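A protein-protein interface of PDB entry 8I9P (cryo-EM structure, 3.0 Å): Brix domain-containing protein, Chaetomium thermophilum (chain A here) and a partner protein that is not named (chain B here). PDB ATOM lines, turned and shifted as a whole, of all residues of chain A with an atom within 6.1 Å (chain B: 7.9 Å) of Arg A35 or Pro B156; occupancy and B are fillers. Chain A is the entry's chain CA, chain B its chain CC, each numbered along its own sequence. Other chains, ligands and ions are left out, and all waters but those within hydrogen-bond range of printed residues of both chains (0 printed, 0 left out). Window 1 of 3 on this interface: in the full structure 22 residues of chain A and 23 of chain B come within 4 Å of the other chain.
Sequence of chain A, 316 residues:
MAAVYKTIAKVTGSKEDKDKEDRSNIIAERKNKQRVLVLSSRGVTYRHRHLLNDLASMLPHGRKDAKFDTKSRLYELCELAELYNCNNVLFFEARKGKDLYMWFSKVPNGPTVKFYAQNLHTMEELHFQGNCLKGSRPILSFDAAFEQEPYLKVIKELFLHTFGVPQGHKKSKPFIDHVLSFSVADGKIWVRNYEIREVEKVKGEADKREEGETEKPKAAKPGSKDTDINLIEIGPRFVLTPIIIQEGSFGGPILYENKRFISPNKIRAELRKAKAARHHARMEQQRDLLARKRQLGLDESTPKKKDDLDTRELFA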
ATOM      1  N   ARG A  23     -13.830   0.479  -4.273  1.00  0.00           N
ATOM      2  CA  ARG A  23     -12.966  -0.232  -3.341  1.00  0.00           C
ATOM      3  C   ARG A  23     -13.758  -0.955  -2.257  1.00  0.00           C
ATOM      4  O   ARG A  23     -13.230  -1.227  -1.174  1.00  0.00           O
ATOM      5  CB  ARG A  23     -11.970   0.745  -2.719  1.00  0.00           C
ATOM      6  CG  ARG A  23     -10.573   0.187  -2.515  1.00  0.00           C
ATOM      7  CD  ARG A  23      -9.650   1.162  -1.776  1.00  0.00           C
ATOM      8  NE  ARG A  23      -9.373   2.390  -2.514  1.00  0.00           N
ATOM      9  CZ  ARG A  23     -10.014   3.539  -2.343  1.00  0.00           C
ATOM     10  NH1 ARG A  23     -10.974   3.669  -1.441  1.00  0.00           N
ATOM     11  NH2 ARG A  23      -9.679   4.587  -3.089  1.00  0.00           N
ATOM     12  N   SER A  24     -15.023  -1.274  -2.536  1.00  0.00           N
ATOM     13  CA  SER A  24     -15.928  -1.867  -1.559  1.00  0.00           C
ATOM     14  C   SER A  24     -15.560  -3.290  -1.164  1.00  0.00           C
ATOM     15  O   SER A  24     -16.065  -3.770  -0.144  1.00  0.00           O
ATOM     16  CB  SER A  24     -17.357  -1.855  -2.105  1.00  0.00           C
ATOM     17  OG  SER A  24     -18.274  -2.317  -1.132  1.00  0.00           O
ATOM     18  N   ASN A  25     -14.720  -3.968  -1.956  1.00  0.00           N
ATOM     19  CA  ASN A  25     -14.306  -5.357  -1.732  1.00  0.00           C
ATOM     20  C   ASN A  25     -15.492  -6.320  -1.706  1.00  0.00           C
ATOM     21  O   ASN A  25     -15.432  -7.373  -1.067  1.00  0.00           O
ATOM     22  CB  ASN A  25     -13.469  -5.504  -0.454  1.00  0.00           C
ATOM     23  CG  ASN A  25     -12.190  -6.281  -0.681  1.00  0.00           C
ATOM     24  OD1 ASN A  25     -11.972  -6.840  -1.756  1.00  0.00           O
ATOM     25  ND2 ASN A  25     -11.335  -6.323   0.334  1.00  0.00           N
ATOM     26  N   LYS A  33     -22.535  -4.234   2.601  1.00  0.00           N
ATOM     27  CA  LYS A  33     -21.307  -3.653   3.142  1.00  0.00           C
ATOM     28  C   LYS A  33     -21.321  -3.796   4.657  1.00  0.00           C
ATOM     29  O   LYS A  33     -21.884  -2.959   5.366  1.00  0.00           O
ATOM     30  CB  LYS A  33     -21.185  -2.190   2.732  1.00  0.00           C
ATOM     31  CG  LYS A  33     -21.117  -1.954   1.234  1.00  0.00           C
ATOM     32  CD  LYS A  33     -20.248  -0.752   0.905  1.00  0.00           C
ATOM     33  CE  LYS A  33     -20.748   0.499   1.601  1.00  0.00           C
ATOM     34  NZ  LYS A  33     -22.077   0.925   1.084  1.00  0.00           N
ATOM     35  N   GLN A  34     -20.709  -4.864   5.161  1.00  0.00           N
ATOM     36  CA  GLN A  34     -20.689  -5.144   6.589  1.00  0.00           C
ATOM     37  C   GLN A  34     -19.248  -5.358   7.030  1.00  0.00           C
ATOM     38  O   GLN A  34     -18.527  -6.155   6.423  1.00  0.00           O
ATOM     39  CB  GLN A  34     -21.538  -6.383   6.914  1.00  0.00           C
ATOM     40  CG  GLN A  34     -23.085  -6.211   7.018  1.00  0.00           C
ATOM     41  CD  GLN A  34     -23.614  -4.855   7.504  1.00  0.00           C
ATOM     42  OE1 GLN A  34     -23.027  -4.256   8.405  1.00  0.00           O
ATOM     43  NE2 GLN A  34     -24.615  -4.307   6.822  1.00  0.00           N
ATOM     44  N   ARG A  35     -18.827  -4.648   8.079  1.00  0.00           N
ATOM     45  CA  ARG A  35     -17.492  -4.802   8.643  1.00  0.00           C
ATOM     46  C   ARG A  35     -17.576  -4.895  10.160  1.00  0.00           C
ATOM     47  O   ARG A  35     -18.304  -4.131  10.799  1.00  0.00           O
ATOM     48  CB  ARG A  35     -16.571  -3.641   8.247  1.00  0.00           C
ATOM     49  CG  ARG A  35     -15.742  -3.903   6.999  1.00  0.00           C
ATOM     50  CD  ARG A  35     -14.522  -2.994   6.936  1.00  0.00           C
ATOM     51  NE  ARG A  35     -13.322  -3.641   7.452  1.00  0.00           N
ATOM     52  CZ  ARG A  35     -12.094  -3.156   7.320  1.00  0.00           C
ATOM     53  NH1 ARG A  35     -11.869  -2.003   6.710  1.00  0.00           N
ATOM     54  NH2 ARG A  35     -11.068  -3.844   7.813  1.00  0.00           N
ATOM     55  N   VAL A  36     -16.813  -5.822  10.731  1.00  0.00           N
ATOM     56  CA  VAL A  36     -16.842  -6.119  12.158  1.00  0.00           C
ATOM     57  C   VAL A  36     -15.481  -5.783  12.754  1.00  0.00           C
ATOM     58  O   VAL A  36     -14.444  -6.015  12.125  1.00  0.00           O
ATOM     59  CB  VAL A  36     -17.211  -7.597  12.410  1.00  0.00           C
ATOM     60  CG1 VAL A  36     -17.421  -7.870  13.892  1.00  0.00           C
ATOM     61  CG2 VAL A  36     -18.457  -7.971  11.628  1.00  0.00           C
ATOM     62  N   LEU A  37     -15.495  -5.215  13.968  1.00  0.00           N
ATOM     63  CA  LEU A  37     -14.232  -4.949  14.710  1.00  0.00           C
ATOM     64  C   LEU A  37     -14.262  -5.814  15.968  1.00  0.00           C
ATOM     65  O   LEU A  37     -15.065  -5.518  16.872  1.00  0.00           O
ATOM     66  CB  LEU A  37     -14.110  -3.467  15.073  1.00  0.00           C
ATOM     67  CG  LEU A  37     -12.859  -3.114  15.879  1.00  0.00           C
ATOM     68  CD1 LEU A  37     -11.596  -3.453  15.102  1.00  0.00           C
ATOM     69  CD2 LEU A  37     -12.859  -1.652  16.288  1.00  0.00           C
ATOM     70  N   HIS A  61     -14.648 -10.440   7.082  1.00  0.00           N
ATOM     71  CA  HIS A  61     -14.870  -9.006   7.199  1.00  0.00           C
ATOM     72  C   HIS A  61     -14.664  -8.489   8.619  1.00  0.00           C
ATOM     73  O   HIS A  61     -15.114  -7.382   8.938  1.00  0.00           O
ATOM     74  CB  HIS A  61     -16.278  -8.659   6.708  1.00  0.00           C
ATOM     75  CG  HIS A  61     -17.374  -9.292   7.514  1.00  0.00           C
ATOM     76  ND1 HIS A  61     -17.449 -10.651   7.729  1.00  0.00           N
ATOM     77  CD2 HIS A  61     -18.437  -8.753   8.155  1.00  0.00           C
ATOM     78  CE1 HIS A  61     -18.508 -10.923   8.469  1.00  0.00           C
ATOM     79  NE2 HIS A  61     -19.126  -9.788   8.741  1.00  0.00           N
ATOM     80  N   GLY A  62     -13.988  -9.252   9.462  1.00  0.00           N
ATOM     81  CA  GLY A  62     -13.705  -8.841  10.828  1.00  0.00           C
ATOM     82  C   GLY A  62     -12.223  -8.595  11.016  1.00  0.00           C
ATOM     83  O   GLY A  62     -11.392  -9.312  10.456  1.00  0.00           O
ATOM     84  N   ARG A  63     -11.899  -7.574  11.802  1.00  0.00           N
ATOM     85  CA  ARG A  63     -10.527  -7.254  12.160  1.00  0.00           C
ATOM     86  C   ARG A  63     -10.321  -7.519  13.643  1.00  0.00           C
ATOM     87  O   ARG A  63     -11.215  -7.271  14.457  1.00  0.00           O
ATOM     88  CB  ARG A  63     -10.192  -5.795  11.836  1.00  0.00           C
ATOM     89  CG  ARG A  63      -8.701  -5.498  11.824  1.00  0.00           C
ATOM     90  CD  ARG A  63      -8.410  -4.062  11.396  1.00  0.00           C
ATOM     91  NE  ARG A  63      -7.120  -3.909  10.731  1.00  0.00           N
ATOM     92  CZ  ARG A  63      -5.932  -4.061  11.306  1.00  0.00           C
ATOM     93  NH1 ARG A  63      -5.810  -4.276  12.607  1.00  0.00           N
ATOM     94  NH2 ARG A  63      -4.835  -3.970  10.561  1.00  0.00           N
ATOM     95  N   TYR A  84     -11.055   1.918  11.512  1.00  0.00           N
ATOM     96  CA  TYR A  84     -10.966   0.726  10.625  1.00  0.00           C
ATOM     97  C   TYR A  84     -12.215   0.622   9.738  1.00  0.00           C
ATOM     98  O   TYR A  84     -12.483  -0.487   9.242  1.00  0.00           O
ATOM     99  CB  TYR A  84     -10.742  -0.531  11.470  1.00  0.00           C
ATOM    100  CG  TYR A  84      -9.550  -0.455  12.390  1.00  0.00           C
ATOM    101  CD1 TYR A  84      -8.264  -0.374  11.886  1.00  0.00           C
ATOM    102  CD2 TYR A  84      -9.707  -0.465  13.765  1.00  0.00           C
ATOM    103  CE1 TYR A  84      -7.163  -0.306  12.724  1.00  0.00           C
ATOM    104  CE2 TYR A  84      -8.618  -0.397  14.617  1.00  0.00           C
ATOM    105  CZ  TYR A  84      -7.340  -0.316  14.095  1.00  0.00           C
ATOM    106  OH  TYR A  84      -6.260  -0.248  14.926  1.00  0.00           O
ATOM    107  N   ASN A  85     -12.944   1.725   9.547  1.00  0.00           N
ATOM    108  CA  ASN A  85     -14.130   1.758   8.679  1.00  0.00           C
ATOM    109  C   ASN A  85     -15.091   0.610   8.984  1.00  0.00           C
ATOM    110  O   ASN A  85     -15.650  -0.013   8.081  1.00  0.00           O
ATOM    111  CB  ASN A  85     -13.739   1.763   7.198  1.00  0.00           C
ATOM    112  CG  ASN A  85     -13.285   3.124   6.718  1.00  0.00           C
ATOM    113  OD1 ASN A  85     -12.739   3.914   7.486  1.00  0.00           O
ATOM    114  ND2 ASN A  85     -13.508   3.405   5.441  1.00  0.00           N
ATOM    115  N   CYS A  86     -15.283   0.327  10.267  1.00  0.00           N
ATOM    116  CA  CYS A  86     -16.160  -0.747  10.705  1.00  0.00           C
ATOM    117  C   CYS A  86     -17.486  -0.185  11.203  1.00  0.00           C
ATOM    118  O   CYS A  86     -17.538   0.884  11.816  1.00  0.00           O
ATOM    119  CB  CYS A  86     -15.498  -1.571  11.811  1.00  0.00           C
ATOM    120  SG  CYS A  86     -14.030  -2.491  11.292  1.00  0.00           S
ATOM    121  N   ASN A  87     -18.565  -0.920  10.928  1.00  0.00           N
ATOM    122  CA  ASN A  87     -19.887  -0.569  11.431  1.00  0.00           C
ATOM    123  C   ASN A  87     -20.439  -1.616  12.392  1.00  0.00           C
ATOM    124  O   ASN A  87     -21.615  -1.538  12.766  1.00  0.00           O
ATOM    125  CB  ASN A  87     -20.870  -0.343  10.276  1.00  0.00           C
ATOM    126  CG  ASN A  87     -20.873  -1.481   9.275  1.00  0.00           C
ATOM    127  OD1 ASN A  87     -20.057  -2.396   9.355  1.00  0.00           O
ATOM    128  ND2 ASN A  87     -21.797  -1.428   8.325  1.00  0.00           N
ATOM    129  N   ASN A  88     -19.623  -2.584  12.804  1.00  0.00           N
ATOM    130  CA  ASN A  88     -20.011  -3.554  13.824  1.00  0.00           C
ATOM    131  C   ASN A  88     -18.851  -3.704  14.790  1.00  0.00           C
ATOM    132  O   ASN A  88     -17.694  -3.763  14.362  1.00  0.00           O
ATOM    133  CB  ASN A  88     -20.363  -4.910  13.211  1.00  0.00           C
ATOM    134  CG  ASN A  88     -21.665  -4.889  12.453  1.00  0.00           C
ATOM    135  OD1 ASN A  88     -22.742  -4.961  13.042  1.00  0.00           O
ATOM    136  ND2 ASN A  88     -21.577  -4.799  11.135  1.00  0.00           N
ATOM    137  N   VAL A  89     -19.150  -3.759  16.084  1.00  0.00           N
ATOM    138  CA  VAL A  89     -18.149  -4.045  17.102  1.00  0.00           C
ATOM    139  C   VAL A  89     -18.628  -5.204  17.962  1.00  0.00           C
ATOM    140  O   VAL A  89     -19.804  -5.264  18.352  1.00  0.00           O
ATOM    141  CB  VAL A  89     -17.812  -2.809  17.956  1.00  0.00           C
ATOM    142  CG1 VAL A  89     -16.946  -1.855  17.167  1.00  0.00           C
ATOM    143  CG2 VAL A  89     -19.068  -2.102  18.366  1.00  0.00           C
ATOM    144  N   HIS A 161     -26.149  -9.456  11.118  1.00  0.00           N
ATOM    145  CA  HIS A 161     -25.226  -8.449  10.594  1.00  0.00           C
ATOM    146  C   HIS A 161     -23.801  -8.655  11.097  1.00  0.00           C
ATOM    147  O   HIS A 161     -22.845  -8.117  10.542  1.00  0.00           O
ATOM    148  CB  HIS A 161     -25.730  -7.055  10.944  1.00  0.00           C
ATOM    149  CG  HIS A 161     -26.746  -6.523   9.984  1.00  0.00           C
ATOM    150  ND1 HIS A 161     -27.317  -5.276  10.118  1.00  0.00           N
ATOM    151  CD2 HIS A 161     -27.291  -7.068   8.870  1.00  0.00           C
ATOM    152  CE1 HIS A 161     -28.171  -5.077   9.130  1.00  0.00           C
ATOM    153  NE2 HIS A 161     -28.174  -6.149   8.360  1.00  0.00           N
ATOM    154  N   HIS A 169     -17.237 -10.728  -0.897  1.00  0.00           N
ATOM    155  CA  HIS A 169     -16.026 -10.505  -0.124  1.00  0.00           C
ATOM    156  C   HIS A 169     -15.020 -11.598  -0.463  1.00  0.00           C
ATOM    157  O   HIS A 169     -15.231 -12.769  -0.145  1.00  0.00           O
ATOM    158  CB  HIS A 169     -16.370 -10.518   1.366  1.00  0.00           C
ATOM    159  CG  HIS A 169     -15.376  -9.810   2.231  1.00  0.00           C
ATOM    160  ND1 HIS A 169     -14.068 -10.218   2.361  1.00  0.00           N
ATOM    161  CD2 HIS A 169     -15.513  -8.722   3.025  1.00  0.00           C
ATOM    162  CE1 HIS A 169     -13.438  -9.407   3.191  1.00  0.00           C
ATOM    163  NE2 HIS A 169     -14.292  -8.490   3.608  1.00  0.00           N
ATOM    164  N   GLU B 153     -23.017   8.194   9.008  1.00  0.00           N
ATOM    165  CA  GLU B 153     -22.885   6.749   8.942  1.00  0.00           C
ATOM    166  C   GLU B 153     -21.518   6.359   8.383  1.00  0.00           C
ATOM    167  O   GLU B 153     -20.908   7.075   7.585  1.00  0.00           O
ATOM    168  CB  GLU B 153     -24.000   6.147   8.090  1.00  0.00           C
ATOM    169  CG  GLU B 153     -24.506   4.806   8.595  1.00  0.00           C
ATOM    170  CD  GLU B 153     -25.673   4.948   9.553  1.00  0.00           C
ATOM    171  OE1 GLU B 153     -26.773   5.325   9.098  1.00  0.00           O
ATOM    172  OE2 GLU B 153     -25.491   4.684  10.759  1.00  0.00           O
ATOM    173  N   ILE B 154     -21.040   5.198   8.819  1.00  0.00           N
ATOM    174  CA  ILE B 154     -19.730   4.690   8.435  1.00  0.00           C
ATOM    175  C   ILE B 154     -19.905   3.750   7.254  1.00  0.00           C
ATOM    176  O   ILE B 154     -20.635   2.755   7.345  1.00  0.00           O
ATOM    177  CB  ILE B 154     -19.043   3.974   9.610  1.00  0.00           C
ATOM    178  CG1 ILE B 154     -18.558   4.991  10.643  1.00  0.00           C
ATOM    179  CG2 ILE B 154     -17.879   3.122   9.116  1.00  0.00           C
ATOM    180  CD1 ILE B 154     -17.803   4.373  11.795  1.00  0.00           C
ATOM    181  N   ASP B 155     -19.252   4.071   6.140  1.00  0.00           N
ATOM    182  CA  ASP B 155     -19.204   3.149   5.018  1.00  0.00           C
ATOM    183  C   ASP B 155     -18.054   2.153   5.146  1.00  0.00           C
ATOM    184  O   ASP B 155     -16.947   2.538   5.547  1.00  0.00           O
ATOM    185  CB  ASP B 155     -19.178   3.905   3.675  1.00  0.00           C
ATOM    186  CG  ASP B 155     -17.900   4.728   3.408  1.00  0.00           C
ATOM    187  OD1 ASP B 155     -16.970   4.830   4.228  1.00  0.00           O
ATOM    188  OD2 ASP B 155     -17.836   5.304   2.302  1.00  0.00           O
ATOM    189  N   PRO B 156     -18.302   0.861   4.967  1.00  0.00           N
ATOM    190  CA  PRO B 156     -17.222  -0.122   5.121  1.00  0.00           C
ATOM    191  C   PRO B 156     -16.368  -0.279   3.876  1.00  0.00           C
ATOM    192  O   PRO B 156     -16.288  -1.372   3.307  1.00  0.00           O
ATOM    193  CB  PRO B 156     -17.975  -1.420   5.443  1.00  0.00           C
ATOM    194  CG  PRO B 156     -19.319  -0.979   5.920  1.00  0.00           C
ATOM    195  CD  PRO B 156     -19.625   0.239   5.113  1.00  0.00           C
ATOM    196  N   VAL B 157     -15.723   0.796   3.445  1.00  0.00           N
ATOM    197  CA  VAL B 157     -14.786   0.747   2.331  1.00  0.00           C
ATOM    198  C   VAL B 157     -13.380   0.606   2.891  1.00  0.00           C
ATOM    199  O   VAL B 157     -12.981   1.313   3.823  1.00  0.00           O
ATOM    200  CB  VAL B 157     -14.907   1.989   1.425  1.00  0.00           C
ATOM    201  CG1 VAL B 157     -14.352   1.691   0.048  1.00  0.00           C
ATOM    202  CG2 VAL B 157     -16.357   2.408   1.313  1.00  0.00           C
ATOM    203  N   TYR B 158     -12.625  -0.326   2.319  1.00  0.00           N
ATOM    204  CA  TYR B 158     -11.309  -0.671   2.838  1.00  0.00           C
ATOM    205  C   TYR B 158     -10.317   0.435   2.501  1.00  0.00           C
ATOM    206  O   TYR B 158     -10.314   0.956   1.384  1.00  0.00           O
ATOM    207  CB  TYR B 158     -10.837  -2.009   2.264  1.00  0.00           C
ATOM    208  CG  TYR B 158     -11.456  -3.249   2.897  1.00  0.00           C
ATOM    209  CD1 TYR B 158     -12.799  -3.286   3.261  1.00  0.00           C
ATOM    210  CD2 TYR B 158     -10.691  -4.384   3.125  1.00  0.00           C
ATOM    211  CE1 TYR B 158     -13.357  -4.412   3.831  1.00  0.00           C
ATOM    212  CE2 TYR B 158     -11.245  -5.516   3.698  1.00  0.00           C
ATOM    213  CZ  TYR B 158     -12.576  -5.523   4.047  1.00  0.00           C
ATOM    214  OH  TYR B 158     -13.128  -6.645   4.619  1.00  0.00           O
ATOM    215  N   ASP B 159      -9.484   0.799   3.472  1.00  0.00           N
ATOM    216  CA  ASP B 159      -8.541   1.888   3.272  1.00  0.00           C
ATOM    217  C   ASP B 159      -7.321   1.408   2.486  1.00  0.00           C
ATOM    218  O   ASP B 159      -7.022   0.214   2.409  1.00  0.00           O
ATOM    219  CB  ASP B 159      -8.113   2.480   4.614  1.00  0.00           C
ATOM    220  CG  ASP B 159      -9.000   3.628   5.053  1.00  0.00           C
ATOM    221  OD1 ASP B 159      -9.638   4.255   4.182  1.00  0.00           O
ATOM    222  OD2 ASP B 159      -9.056   3.907   6.269  1.00  0.00           O
ATOM    223  N   ASP B 162      -4.685  -0.391   4.626  1.00  0.00           N
ATOM    224  CA  ASP B 162      -5.099  -1.603   5.315  1.00  0.00           C
ATOM    225  C   ASP B 162      -4.281  -2.799   4.842  1.00  0.00           C
ATOM    226  O   ASP B 162      -3.696  -2.793   3.756  1.00  0.00           O
ATOM    227  CB  ASP B 162      -6.589  -1.856   5.074  1.00  0.00           C
ATOM    228  CG  ASP B 162      -7.200  -2.779   6.107  1.00  0.00           C
ATOM    229  OD1 ASP B 162      -6.550  -3.028   7.144  1.00  0.00           O
ATOM    230  OD2 ASP B 162      -8.332  -3.257   5.882  1.00  0.00           O
ATOM    231  N   THR B 163      -4.247  -3.840   5.676  1.00  0.00           N
ATOM    232  CA  THR B 163      -3.631  -5.114   5.324  1.00  0.00           C
ATOM    233  C   THR B 163      -4.541  -5.988   4.469  1.00  0.00           C
ATOM    234  O   THR B 163      -4.230  -7.162   4.240  1.00  0.00           O
ATOM    235  CB  THR B 163      -3.224  -5.874   6.588  1.00  0.00           C
ATOM    236  OG1 THR B 163      -4.350  -6.605   7.090  1.00  0.00           O
ATOM    237  CG2 THR B 163      -2.734  -4.909   7.659  1.00  0.00           C
ATOM    238  N   ASP B 164      -5.663  -5.428   3.999  1.00  0.00           N
ATOM    239  CA  ASP B 164      -6.592  -6.170   3.155  1.00  0.00           C
ATOM    240  C   ASP B 164      -6.953  -5.382   1.899  1.00  0.00           C
ATOM    241  O   ASP B 164      -7.960  -5.697   1.254  1.00  0.00           O
ATOM    242  CB  ASP B 164      -7.852  -6.502   3.952  1.00  0.00           C
ATOM    243  CG  ASP B 164      -7.828  -7.902   4.521  1.00  0.00           C
ATOM    244  OD1 ASP B 164      -6.868  -8.649   4.235  1.00  0.00           O
ATOM    245  OD2 ASP B 164      -8.755  -8.241   5.284  1.00  0.00           O
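Ser A24 touches Val B157.
O of Lys A33 touches CG of Pro B156 (3.3 Å).
Arg A35 touches Pro B156 (CG to CB, 3.7 Å).
Arg A35 touches Tyr B158 (CD to CE1, 3.6 Å).
His A61 touches Tyr B158 (CA to OH, 3.9 Å).
NH2 of Arg A63 touches CG2 of Thr B163 (3.7 Å).
Asp B155 touches Asn A85.
Pro B156 touches Asn A85 (CA to O, 3.4 Å).
O of Cys A86 touches CD1 of Ile B154, at 3.5 Å.
CG of Pro B156 touches ND2 of Asn A87 (3.5 Å).
Of the printed residues of chain B, Ser A24 touches Val B157.
Of the printed residues of chain B, Asn A25 touches Tyr B158 (3.5 Å) and Asp B164 (3.6 Å).
Of chain B, only Pro B156, Tyr B158 and Asp B162 come within 4 Å of Arg A35.
Val A36 touches none of the printed residues of chain B.
Printed residues of chain B within 4 Å of Asn A87: Pro B156 (3.5 Å).
Asn A88 touches none of the printed residues of chain B.
Of the printed residues of chain A, Pro B156 touches Lys A33 (3.3 Å), Arg A35 (3.7 Å), Asn A85 (3.4 Å) and Asn A87 (3.5 Å).
Of the printed residues of chain A, Asp B159 touches Asn A85.
The nearest residue of chain B that does not touch Arg A35 is Val B157 (4.5 Å).
The nearest printed residue of chain A that does not touch Pro B156 is Gln A34 (4.2 Å).
The nearest printed residue of chain B that does not touch Ser A24 is Pro B156 (4.2 Å).
The guanidinium group of Arg A63 is in salt-bridge range of the side-chain carboxylate of Asp B162 (3.7 Å).
The side-chain amide nitrogen (ND2) of Asn A85 lies within hydrogen-bond range of the backbone carbonyl oxygen (O) of Val B157.
NE2 of His A169 sits at hydrogen-bond distance from OH of Tyr B158 (2.4 Å).
The side-chain carboxylate of Asp B162 lies within salt-bridge range of the guanidinium group of Arg A35 (3.4 Å).
Of the 10 printed residues of chain B, 9 touch a printed residue of chain A.
Hydrophobic or aromatic side chains of chain B within 4 Å of the printed part of chain A: Ile B154, Pro B156, Val B157 and Tyr B158.
Among the printed residues, 20 pairs touch across the chains.
Among the printed residues, Asp or Glu carboxylates within 4 Å of a Lys or Arg side-chain nitrogen of the other chain: Arg A35 with Asp B162 (3.4 Å) and Arg A63 with Asp B162 (3.7 Å).
The backbone carbonyl oxygen (O) of Tyr A84 is in hydrogen-bond range of the side-chain sulfur (SG) of Cys A86, 3.3 Å away.
The backbone carbonyl oxygen (O) of Tyr A84 lies within hydrogen-bond range of the guanidinium group (NH1) of Arg A35 (3.0 Å).
O of His A61 is in hydrogen-bond range of N of Val A36, 2.9 Å away.
N of Arg A63 lies within hydrogen-bond range of O of Val A36, 3.0 Å away.
The backbone carbonyl oxygen (O) of Arg A35 lies close to the side-chain amide oxygen (OD1) of Asn A87 (2.9 Å).
The side-chain amide oxygen (OD1) of Asn A87 is in hydrogen-bond range of the side-chain amide nitrogen (ND2) of Asn A88.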
